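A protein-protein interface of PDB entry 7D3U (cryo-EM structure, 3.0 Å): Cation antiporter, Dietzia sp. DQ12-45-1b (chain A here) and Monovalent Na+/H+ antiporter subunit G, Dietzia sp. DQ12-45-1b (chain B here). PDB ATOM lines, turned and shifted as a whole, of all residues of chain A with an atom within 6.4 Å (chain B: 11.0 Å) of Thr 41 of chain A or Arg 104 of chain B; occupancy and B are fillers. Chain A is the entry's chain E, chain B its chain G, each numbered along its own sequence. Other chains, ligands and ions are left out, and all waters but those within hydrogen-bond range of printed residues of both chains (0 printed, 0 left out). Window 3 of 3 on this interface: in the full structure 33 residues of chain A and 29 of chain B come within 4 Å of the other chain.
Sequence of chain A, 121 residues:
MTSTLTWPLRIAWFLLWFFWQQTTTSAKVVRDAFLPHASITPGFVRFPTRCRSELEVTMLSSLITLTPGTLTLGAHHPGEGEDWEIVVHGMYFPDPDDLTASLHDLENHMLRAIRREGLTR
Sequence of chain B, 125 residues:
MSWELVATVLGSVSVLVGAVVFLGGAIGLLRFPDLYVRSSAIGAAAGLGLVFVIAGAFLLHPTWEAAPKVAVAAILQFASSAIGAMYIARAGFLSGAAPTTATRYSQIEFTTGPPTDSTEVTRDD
OG of Ser 40 of chain B lies within hydrogen-bond range of SD of Met 91 of chain A (2.6 Å).
OH of Tyr 105 of chain B sits at hydrogen-bond distance from O of Phe 93 of chain A (2.8 Å).
Among the printed residues, no Asp or Glu carboxylate lies within 4 Å of a Lys or Arg side-chain nitrogen of the other chain.
No residue of chain B comes within 4 Å of Ser 39 of chain A.
Ile 40 of chain A touches one residue of chain B.
Thr 41 of chain A touches one residue of chain B.
Gly 43 of chain A touches just one residue of chain B: Tyr 105 (3.1 Å).
No residue of chain B comes within 4 Å of Gly 90 of chain A.
Printed residues of chain B within 4 Å of Met 91 of chain A: Val 37 and Ser 40.
Asp 34 of chain B touches none of the printed residues of chain A.
Of the printed residues of chain A, Ser 40 of chain B touches Met 91.
Arg 104 of chain B touches just these residues of chain A: Thr 41 and Pro 42.
The nearest residue of chain B that does not touch Thr 41 of chain A is Ala 102 of chain B (4.5 Å).
The side-chain hydroxyl (OG1) of Thr 41 of chain A lies within hydrogen-bond range of the backbone NH (N) of Phe 93 of chain A, at 3.4 Å.
The backbone carbonyl oxygen (O) of Val 37 of chain B lies within hydrogen-bond range of the side-chain hydroxyl (OG) of Ser 40 of chain B (2.7 Å).
OG of Ser 40 of chain B sits at hydrogen-bond distance from O of Tyr 36 of chain B, 3.2 Å away.
The backbone NH (N) of Gly 43 of chain A is in hydrogen-bond range of the backbone carbonyl oxygen (O) of Gly 90 of chain A, 2.9 Å away.
The backbone carbonyl oxygen (O) of Thr 100 of chain B sits at hydrogen-bond distance from the side-chain hydroxyl (OG1) of Thr 103 of chain B (2.8 Å).
Ile 40 of chain A touches Pro 33 of chain B.
Thr 41 of chain A touches Arg 104 of chain B (CG2 to NH1, 3.3 Å).
Ala 102 of chain B touches Pro 42 of chain A (O to CD, 3.2 Å).
Pro 42 of chain A touches Thr 103 of chain B.
O of Pro 42 of chain A touches N of Arg 104 of chain B, at 3.6 Å.
Gly 43 of chain A touches Tyr 105 of chain B.
CE of Met 91 of chain A touches CG1 of Val 37 of chain B, at 3.7 Å.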
ATOM      1  N   ALA A  38     -16.724  20.718 -11.038  1.00  0.00           N
ATOM      2  CA  ALA A  38     -16.608  20.656 -12.494  1.00  0.00           C
ATOM      3  C   ALA A  38     -15.285  21.228 -12.986  1.00  0.00           C
ATOM      4  O   ALA A  38     -15.042  21.234 -14.197  1.00  0.00           O
ATOM      5  CB  ALA A  38     -17.764  21.362 -13.218  1.00  0.00           C
ATOM      6  N   SER A  39     -14.421  21.701 -12.091  1.00  0.00           N
ATOM      7  CA  SER A  39     -13.069  22.102 -12.439  1.00  0.00           C
ATOM      8  C   SER A  39     -12.047  21.040 -12.074  1.00  0.00           C
ATOM      9  O   SER A  39     -10.862  21.207 -12.372  1.00  0.00           O
ATOM     10  CB  SER A  39     -12.712  23.423 -11.748  1.00  0.00           C
ATOM     11  OG  SER A  39     -11.380  23.800 -12.043  1.00  0.00           O
ATOM     12  N   ILE A  40     -12.478  19.962 -11.430  1.00  0.00           N
ATOM     13  CA  ILE A  40     -11.669  18.765 -11.242  1.00  0.00           C
ATOM     14  C   ILE A  40     -12.205  17.700 -12.188  1.00  0.00           C
ATOM     15  O   ILE A  40     -13.413  17.439 -12.222  1.00  0.00           O
ATOM     16  CB  ILE A  40     -11.688  18.287  -9.779  1.00  0.00           C
ATOM     17  CG1 ILE A  40     -13.109  17.933  -9.341  1.00  0.00           C
ATOM     18  CG2 ILE A  40     -11.113  19.352  -8.862  1.00  0.00           C
ATOM     19  CD1 ILE A  40     -13.182  17.253  -7.992  1.00  0.00           C
ATOM     20  N   THR A  41     -11.311  17.105 -12.973  1.00  0.00           N
ATOM     21  CA  THR A  41     -11.682  16.137 -14.003  1.00  0.00           C
ATOM     22  C   THR A  41     -10.825  14.892 -13.835  1.00  0.00           C
ATOM     23  O   THR A  41      -9.915  14.633 -14.630  1.00  0.00           O
ATOM     24  CB  THR A  41     -11.516  16.741 -15.396  1.00  0.00           C
ATOM     25  OG1 THR A  41     -10.338  17.559 -15.421  1.00  0.00           O
ATOM     26  CG2 THR A  41     -12.714  17.612 -15.730  1.00  0.00           C
ATOM     27  N   PRO A  42     -11.087  14.099 -12.798  1.00  0.00           N
ATOM     28  CA  PRO A  42     -10.217  12.954 -12.511  1.00  0.00           C
ATOM     29  C   PRO A  42     -10.246  11.926 -13.630  1.00  0.00           C
ATOM     30  O   PRO A  42     -11.257  11.733 -14.307  1.00  0.00           O
ATOM     31  CB  PRO A  42     -10.798  12.381 -11.215  1.00  0.00           C
ATOM     32  CG  PRO A  42     -12.191  12.882 -11.164  1.00  0.00           C
ATOM     33  CD  PRO A  42     -12.175  14.224 -11.816  1.00  0.00           C
ATOM     34  N   GLY A  43      -9.111  11.258 -13.812  1.00  0.00           N
ATOM     35  CA  GLY A  43      -8.982  10.234 -14.827  1.00  0.00           C
ATOM     36  C   GLY A  43      -7.862   9.262 -14.529  1.00  0.00           C
ATOM     37  O   GLY A  43      -6.801   9.663 -14.043  1.00  0.00           O
ATOM     38  N   GLY A  90      -5.315  11.159 -12.043  1.00  0.00           N
ATOM     39  CA  GLY A  90      -4.994  12.568 -12.214  1.00  0.00           C
ATOM     40  C   GLY A  90      -6.210  13.461 -12.122  1.00  0.00           C
ATOM     41  O   GLY A  90      -7.241  13.194 -12.735  1.00  0.00           O
ATOM     42  N   MET A  91      -6.074  14.530 -11.343  1.00  0.00           N
ATOM     43  CA  MET A  91      -7.100  15.556 -11.250  1.00  0.00           C
ATOM     44  C   MET A  91      -6.792  16.697 -12.211  1.00  0.00           C
ATOM     45  O   MET A  91      -5.632  16.958 -12.539  1.00  0.00           O
ATOM     46  CB  MET A  91      -7.203  16.094  -9.823  1.00  0.00           C
ATOM     47  CG  MET A  91      -7.054  15.036  -8.750  1.00  0.00           C
ATOM     48  SD  MET A  91      -6.465  15.723  -7.191  1.00  0.00           S
ATOM     49  CE  MET A  91      -7.291  17.311  -7.185  1.00  0.00           C
ATOM     50  N   TYR A  92      -7.849  17.386 -12.636  1.00  0.00           N
ATOM     51  CA  TYR A  92      -7.788  18.472 -13.622  1.00  0.00           C
ATOM     52  C   TYR A  92      -6.807  18.161 -14.750  1.00  0.00           C
ATOM     53  O   TYR A  92      -5.894  18.931 -15.058  1.00  0.00           O
ATOM     54  CB  TYR A  92      -7.472  19.817 -12.963  1.00  0.00           C
ATOM     55  CG  TYR A  92      -6.374  19.818 -11.924  1.00  0.00           C
ATOM     56  CD1 TYR A  92      -5.043  19.968 -12.287  1.00  0.00           C
ATOM     57  CD2 TYR A  92      -6.674  19.701 -10.574  1.00  0.00           C
ATOM     58  CE1 TYR A  92      -4.042  19.980 -11.338  1.00  0.00           C
ATOM     59  CE2 TYR A  92      -5.680  19.714  -9.618  1.00  0.00           C
ATOM     60  CZ  TYR A  92      -4.366  19.854 -10.005  1.00  0.00           C
ATOM     61  OH  TYR A  92      -3.375  19.868  -9.054  1.00  0.00           O
ATOM     62  N   PHE A  93      -7.012  17.005 -15.376  1.00  0.00           N
ATOM     63  CA  PHE A  93      -6.308  16.608 -16.593  1.00  0.00           C
ATOM     64  C   PHE A  93      -7.362  16.069 -17.547  1.00  0.00           C
ATOM     65  O   PHE A  93      -7.571  14.852 -17.638  1.00  0.00           O
ATOM     66  CB  PHE A  93      -5.221  15.572 -16.303  1.00  0.00           C
ATOM     67  CG  PHE A  93      -3.943  16.163 -15.782  1.00  0.00           C
ATOM     68  CD1 PHE A  93      -3.202  17.035 -16.558  1.00  0.00           C
ATOM     69  CD2 PHE A  93      -3.480  15.840 -14.519  1.00  0.00           C
ATOM     70  CE1 PHE A  93      -2.024  17.577 -16.082  1.00  0.00           C
ATOM     71  CE2 PHE A  93      -2.303  16.379 -14.037  1.00  0.00           C
ATOM     72  CZ  PHE A  93      -1.575  17.249 -14.820  1.00  0.00           C
ATOM     73  N   PRO A  94      -8.049  16.951 -18.277  1.00  0.00           N
ATOM     74  CA  PRO A  94      -9.227  16.519 -19.047  1.00  0.00           C
ATOM     75  C   PRO A  94      -8.906  15.658 -20.254  1.00  0.00           C
ATOM     76  O   PRO A  94      -9.839  15.148 -20.885  1.00  0.00           O
ATOM     77  CB  PRO A  94      -9.865  17.844 -19.473  1.00  0.00           C
ATOM     78  CG  PRO A  94      -8.718  18.790 -19.549  1.00  0.00           C
ATOM     79  CD  PRO A  94      -7.765  18.385 -18.456  1.00  0.00           C
ATOM     80  N   ASP A  95      -7.633  15.482 -20.601  1.00  0.00           N
ATOM     81  CA  ASP A  95      -7.240  14.663 -21.742  1.00  0.00           C
ATOM     82  C   ASP A  95      -6.120  13.737 -21.290  1.00  0.00           C
ATOM     83  O   ASP A  95      -5.087  14.222 -20.784  1.00  0.00           O
ATOM     84  CB  ASP A  95      -6.798  15.529 -22.922  1.00  0.00           C
ATOM     85  CG  ASP A  95      -7.954  16.260 -23.572  1.00  0.00           C
ATOM     86  OD1 ASP A  95      -9.117  15.892 -23.308  1.00  0.00           O
ATOM     87  OD2 ASP A  95      -7.701  17.207 -24.347  1.00  0.00           O
ATOM     88  N   ARG B  31     -14.669  18.967   0.509  1.00  0.00           N
ATOM     89  CA  ARG B  31     -15.224  19.300  -0.802  1.00  0.00           C
ATOM     90  C   ARG B  31     -14.502  18.576  -1.933  1.00  0.00           C
ATOM     91  O   ARG B  31     -14.087  19.195  -2.909  1.00  0.00           O
ATOM     92  CB  ARG B  31     -15.187  20.808  -1.011  1.00  0.00           C
ATOM     93  CG  ARG B  31     -13.847  21.448  -0.702  1.00  0.00           C
ATOM     94  CD  ARG B  31     -13.823  22.891  -1.154  1.00  0.00           C
ATOM     95  NE  ARG B  31     -14.683  23.104  -2.313  1.00  0.00           N
ATOM     96  CZ  ARG B  31     -15.112  24.295  -2.718  1.00  0.00           C
ATOM     97  NH1 ARG B  31     -14.759  25.388  -2.056  1.00  0.00           N
ATOM     98  NH2 ARG B  31     -15.893  24.394  -3.782  1.00  0.00           N
ATOM     99  N   PHE B  32     -14.366  17.255  -1.836  1.00  0.00           N
ATOM    100  CA  PHE B  32     -13.807  16.449  -2.913  1.00  0.00           C
ATOM    101  C   PHE B  32     -14.698  15.228  -3.097  1.00  0.00           C
ATOM    102  O   PHE B  32     -15.000  14.528  -2.115  1.00  0.00           O
ATOM    103  CB  PHE B  32     -12.362  16.023  -2.623  1.00  0.00           C
ATOM    104  CG  PHE B  32     -11.331  17.025  -3.064  1.00  0.00           C
ATOM    105  CD1 PHE B  32     -11.625  17.958  -4.039  1.00  0.00           C
ATOM    106  CD2 PHE B  32     -10.066  17.028  -2.508  1.00  0.00           C
ATOM    107  CE1 PHE B  32     -10.683  18.879  -4.442  1.00  0.00           C
ATOM    108  CE2 PHE B  32      -9.120  17.947  -2.908  1.00  0.00           C
ATOM    109  CZ  PHE B  32      -9.429  18.871  -3.877  1.00  0.00           C
ATOM    110  N   PRO B  33     -15.133  14.933  -4.324  1.00  0.00           N
ATOM    111  CA  PRO B  33     -16.156  13.889  -4.489  1.00  0.00           C
ATOM    112  C   PRO B  33     -15.623  12.477  -4.338  1.00  0.00           C
ATOM    113  O   PRO B  33     -16.305  11.624  -3.758  1.00  0.00           O
ATOM    114  CB  PRO B  33     -16.682  14.151  -5.906  1.00  0.00           C
ATOM    115  CG  PRO B  33     -15.516  14.740  -6.623  1.00  0.00           C
ATOM    116  CD  PRO B  33     -14.738  15.538  -5.608  1.00  0.00           C
ATOM    117  N   ASP B  34     -14.426  12.203  -4.836  1.00  0.00           N
ATOM    118  CA  ASP B  34     -13.913  10.846  -4.923  1.00  0.00           C
ATOM    119  C   ASP B  34     -13.061  10.492  -3.711  1.00  0.00           C
ATOM    120  O   ASP B  34     -12.706  11.340  -2.889  1.00  0.00           O
ATOM    121  CB  ASP B  34     -13.091  10.673  -6.201  1.00  0.00           C
ATOM    122  CG  ASP B  34     -13.377   9.369  -6.902  1.00  0.00           C
ATOM    123  OD1 ASP B  34     -13.638   8.369  -6.203  1.00  0.00           O
ATOM    124  OD2 ASP B  34     -13.344   9.342  -8.150  1.00  0.00           O
ATOM    125  N   TYR B  36     -10.208   8.898  -4.634  1.00  0.00           N
ATOM    126  CA  TYR B  36      -8.920   9.025  -5.300  1.00  0.00           C
ATOM    127  C   TYR B  36      -8.489  10.480  -5.400  1.00  0.00           C
ATOM    128  O   TYR B  36      -7.294  10.780  -5.318  1.00  0.00           O
ATOM    129  CB  TYR B  36      -8.992   8.376  -6.679  1.00  0.00           C
ATOM    130  CG  TYR B  36      -9.663   7.025  -6.640  1.00  0.00           C
ATOM    131  CD1 TYR B  36      -8.979   5.903  -6.201  1.00  0.00           C
ATOM    132  CD2 TYR B  36     -10.987   6.877  -7.019  1.00  0.00           C
ATOM    133  CE1 TYR B  36      -9.588   4.673  -6.154  1.00  0.00           C
ATOM    134  CE2 TYR B  36     -11.605   5.650  -6.974  1.00  0.00           C
ATOM    135  CZ  TYR B  36     -10.902   4.552  -6.540  1.00  0.00           C
ATOM    136  OH  TYR B  36     -11.515   3.324  -6.494  1.00  0.00           O
ATOM    137  N   VAL B  37      -9.441  11.397  -5.574  1.00  0.00           N
ATOM    138  CA  VAL B  37      -9.120  12.817  -5.471  1.00  0.00           C
ATOM    139  C   VAL B  37      -8.671  13.149  -4.055  1.00  0.00           C
ATOM    140  O   VAL B  37      -7.691  13.878  -3.848  1.00  0.00           O
ATOM    141  CB  VAL B  37     -10.327  13.671  -5.899  1.00  0.00           C
ATOM    142  CG1 VAL B  37      -9.999  15.143  -5.779  1.00  0.00           C
ATOM    143  CG2 VAL B  37     -10.736  13.332  -7.316  1.00  0.00           C
ATOM    144  N   SER B  40      -5.202  11.760  -3.597  1.00  0.00           N
ATOM    145  CA  SER B  40      -4.238  12.528  -4.376  1.00  0.00           C
ATOM    146  C   SER B  40      -3.930  13.863  -3.717  1.00  0.00           C
ATOM    147  O   SER B  40      -2.799  14.354  -3.811  1.00  0.00           O
ATOM    148  CB  SER B  40      -4.764  12.748  -5.794  1.00  0.00           C
ATOM    149  OG  SER B  40      -5.900  13.591  -5.787  1.00  0.00           O
ATOM    150  N   PRO B  99     -15.670   5.455  -8.160  1.00  0.00           N
ATOM    151  CA  PRO B  99     -15.168   6.764  -8.585  1.00  0.00           C
ATOM    152  C   PRO B  99     -16.316   7.722  -8.856  1.00  0.00           C
ATOM    153  O   PRO B  99     -17.446   7.320  -9.141  1.00  0.00           O
ATOM    154  CB  PRO B  99     -14.391   6.449  -9.864  1.00  0.00           C
ATOM    155  CG  PRO B  99     -15.038   5.219 -10.390  1.00  0.00           C
ATOM    156  CD  PRO B  99     -15.453   4.422  -9.185  1.00  0.00           C
ATOM    157  N   THR B 100     -16.007   9.012  -8.754  1.00  0.00           N
ATOM    158  CA  THR B 100     -17.027  10.036  -8.919  1.00  0.00           C
ATOM    159  C   THR B 100     -17.657   9.952 -10.305  1.00  0.00           C
ATOM    160  O   THR B 100     -17.055   9.466 -11.265  1.00  0.00           O
ATOM    161  CB  THR B 100     -16.436  11.428  -8.710  1.00  0.00           C
ATOM    162  OG1 THR B 100     -15.918  11.528  -7.378  1.00  0.00           O
ATOM    163  CG2 THR B 100     -17.502  12.488  -8.901  1.00  0.00           C
ATOM    164  N   THR B 101     -18.895  10.440 -10.398  1.00  0.00           N
ATOM    165  CA  THR B 101     -19.594  10.445 -11.675  1.00  0.00           C
ATOM    166  C   THR B 101     -18.918  11.340 -12.702  1.00  0.00           C
ATOM    167  O   THR B 101     -19.156  11.174 -13.902  1.00  0.00           O
ATOM    168  CB  THR B 101     -21.043  10.888 -11.480  1.00  0.00           C
ATOM    169  OG1 THR B 101     -21.711   9.971 -10.605  1.00  0.00           O
ATOM    170  CG2 THR B 101     -21.767  10.927 -12.813  1.00  0.00           C
ATOM    171  N   ALA B 102     -18.088  12.280 -12.261  1.00  0.00           N
ATOM    172  CA  ALA B 102     -17.368  13.172 -13.168  1.00  0.00           C
ATOM    173  C   ALA B 102     -15.959  12.646 -13.430  1.00  0.00           C
ATOM    174  O   ALA B 102     -14.956  13.264 -13.078  1.00  0.00           O
ATOM    175  CB  ALA B 102     -17.332  14.587 -12.599  1.00  0.00           C
ATOM    176  N   THR B 103     -15.896  11.477 -14.062  1.00  0.00           N
ATOM    177  CA  THR B 103     -14.638  10.860 -14.467  1.00  0.00           C
ATOM    178  C   THR B 103     -14.653  10.746 -15.984  1.00  0.00           C
ATOM    179  O   THR B 103     -15.306   9.854 -16.537  1.00  0.00           O
ATOM    180  CB  THR B 103     -14.450   9.495 -13.814  1.00  0.00           C
ATOM    181  OG1 THR B 103     -14.479   9.640 -12.389  1.00  0.00           O
ATOM    182  CG2 THR B 103     -13.121   8.896 -14.222  1.00  0.00           C
ATOM    183  N   ARG B 104     -13.934  11.648 -16.651  1.00  0.00           N
ATOM    184  CA  ARG B 104     -14.030  11.750 -18.102  1.00  0.00           C
ATOM    185  C   ARG B 104     -13.469  10.512 -18.791  1.00  0.00           C
ATOM    186  O   ARG B 104     -13.979  10.091 -19.834  1.00  0.00           O
ATOM    187  CB  ARG B 104     -13.306  13.006 -18.583  1.00  0.00           C
ATOM    188  CG  ARG B 104     -14.133  14.272 -18.463  1.00  0.00           C
ATOM    189  CD  ARG B 104     -13.251  15.504 -18.530  1.00  0.00           C
ATOM    190  NE  ARG B 104     -13.825  16.562 -19.357  1.00  0.00           N
ATOM    191  CZ  ARG B 104     -14.795  17.380 -18.960  1.00  0.00           C
ATOM    192  NH1 ARG B 104     -15.306  17.267 -17.741  1.00  0.00           N
ATOM    193  NH2 ARG B 104     -15.254  18.314 -19.782  1.00  0.00           N
ATOM    194  N   TYR B 105     -12.427   9.912 -18.223  1.00  0.00           N
ATOM    195  CA  TYR B 105     -11.767   8.779 -18.856  1.00  0.00           C
ATOM    196  C   TYR B 105     -11.158   7.899 -17.780  1.00  0.00           C
ATOM    197  O   TYR B 105     -10.584   8.407 -16.815  1.00  0.00           O
ATOM    198  CB  TYR B 105     -10.682   9.246 -19.829  1.00  0.00           C
ATOM    199  CG  TYR B 105      -9.590  10.051 -19.165  1.00  0.00           C
ATOM    200  CD1 TYR B 105      -9.771  11.396 -18.880  1.00  0.00           C
ATOM    201  CD2 TYR B 105      -8.384   9.464 -18.812  1.00  0.00           C
ATOM    202  CE1 TYR B 105      -8.782  12.132 -18.270  1.00  0.00           C
ATOM    203  CE2 TYR B 105      -7.389  10.194 -18.200  1.00  0.00           C
ATOM    204  CZ  TYR B 105      -7.592  11.528 -17.933  1.00  0.00           C
ATOM    205  OH  TYR B 105      -6.605  12.264 -17.324  1.00  0.00           O
ATOM    206  N   SER B 106     -11.286   6.587 -17.945  1.00  0.00           N
ATOM    207  CA  SER B 106     -10.673   5.631 -17.030  1.00  0.00           C
ATOM    208  C   SER B 106     -10.220   4.430 -17.844  1.00  0.00           C
ATOM    209  O   SER B 106     -11.053   3.693 -18.381  1.00  0.00           O
ATOM    210  CB  SER B 106     -11.643   5.212 -15.927  1.00  0.00           C
ATOM    211  OG  SER B 106     -12.755   4.522 -16.466  1.00  0.00           O
ATOM    212  N   GLN B 107      -8.906   4.236 -17.939  1.00  0.00           N
ATOM    213  CA  GLN B 107      -8.337   3.086 -18.622  1.00  0.00           C
ATOM    214  C   GLN B 107      -8.162   1.893 -17.696  1.00  0.00           C
ATOM    215  O   GLN B 107      -7.351   1.006 -17.983  1.00  0.00           O
ATOM    216  CB  GLN B 107      -7.001   3.464 -19.262  1.00  0.00           C
ATOM    217  CG  GLN B 107      -7.104   4.623 -20.234  1.00  0.00           C
ATOM    218  CD  GLN B 107      -5.754   5.114 -20.704  1.00  0.00           C
ATOM    219  OE1 GLN B 107      -4.722   4.761 -20.139  1.00  0.00           O
ATOM    220  NE2 GLN B 107      -5.756   5.932 -21.748  1.00  0.00           N
ATOM    221  N   ILE B 108      -8.906   1.856 -16.594  1.00  0.00           N
ATOM    222  CA  ILE B 108      -8.871   0.761 -15.634  1.00  0.00           C
ATOM    223  C   ILE B 108     -10.309   0.375 -15.330  1.00  0.00           C
ATOM    224  O   ILE B 108     -11.099   1.215 -14.883  1.00  0.00           O
ATOM    225  CB  ILE B 108      -8.134   1.150 -14.343  1.00  0.00           C
ATOM    226  CG1 ILE B 108      -6.666   1.437 -14.639  1.00  0.00           C
ATOM    227  CG2 ILE B 108      -8.241   0.043 -13.324  1.00  0.00           C
ATOM    228  CD1 ILE B 108      -5.922   0.234 -15.130  1.00  0.00           C
ATOM    229  N   GLU B 109     -10.651  -0.888 -15.569  1.00  0.00           N
ATOM    230  CA  GLU B 109     -12.018  -1.333 -15.355  1.00  0.00           C
ATOM    231  C   GLU B 109     -12.308  -1.490 -13.868  1.00  0.00           C
ATOM    232  O   GLU B 109     -11.423  -1.801 -13.068  1.00  0.00           O
ATOM    233  CB  GLU B 109     -12.270  -2.653 -16.082  1.00  0.00           C
ATOM    234  CG  GLU B 109     -12.112  -2.569 -17.591  1.00  0.00           C
ATOM    235  CD  GLU B 109     -13.166  -1.695 -18.247  1.00  0.00           C
ATOM    236  OE1 GLU B 109     -13.036  -0.453 -18.196  1.00  0.00           O
ATOM    237  OE2 GLU B 109     -14.127  -2.253 -18.815  1.00  0.00           O
ATOM    238  N   PHE B 110     -13.567  -1.272 -13.503  1.00  0.00           N
ATOM    239  CA  PHE B 110     -14.000  -1.316 -12.113  1.00  0.00           C
ATOM    240  C   PHE B 110     -14.896  -2.500 -11.794  1.00  0.00           C
ATOM    241  O   PHE B 110     -14.769  -3.082 -10.716  1.00  0.00           O
ATOM    242  CB  PHE B 110     -14.732  -0.020 -11.750  1.00  0.00           C
ATOM    243  CG  PHE B 110     -13.820   1.154 -11.557  1.00  0.00           C
ATOM    244  CD1 PHE B 110     -13.401   1.908 -12.639  1.00  0.00           C
ATOM    245  CD2 PHE B 110     -13.380   1.504 -10.293  1.00  0.00           C
ATOM    246  CE1 PHE B 110     -12.561   2.990 -12.463  1.00  0.00           C
ATOM    247  CE2 PHE B 110     -12.542   2.585 -10.112  1.00  0.00           C
ATOM    248  CZ  PHE B 110     -12.130   3.327 -11.198  1.00  0.00           C
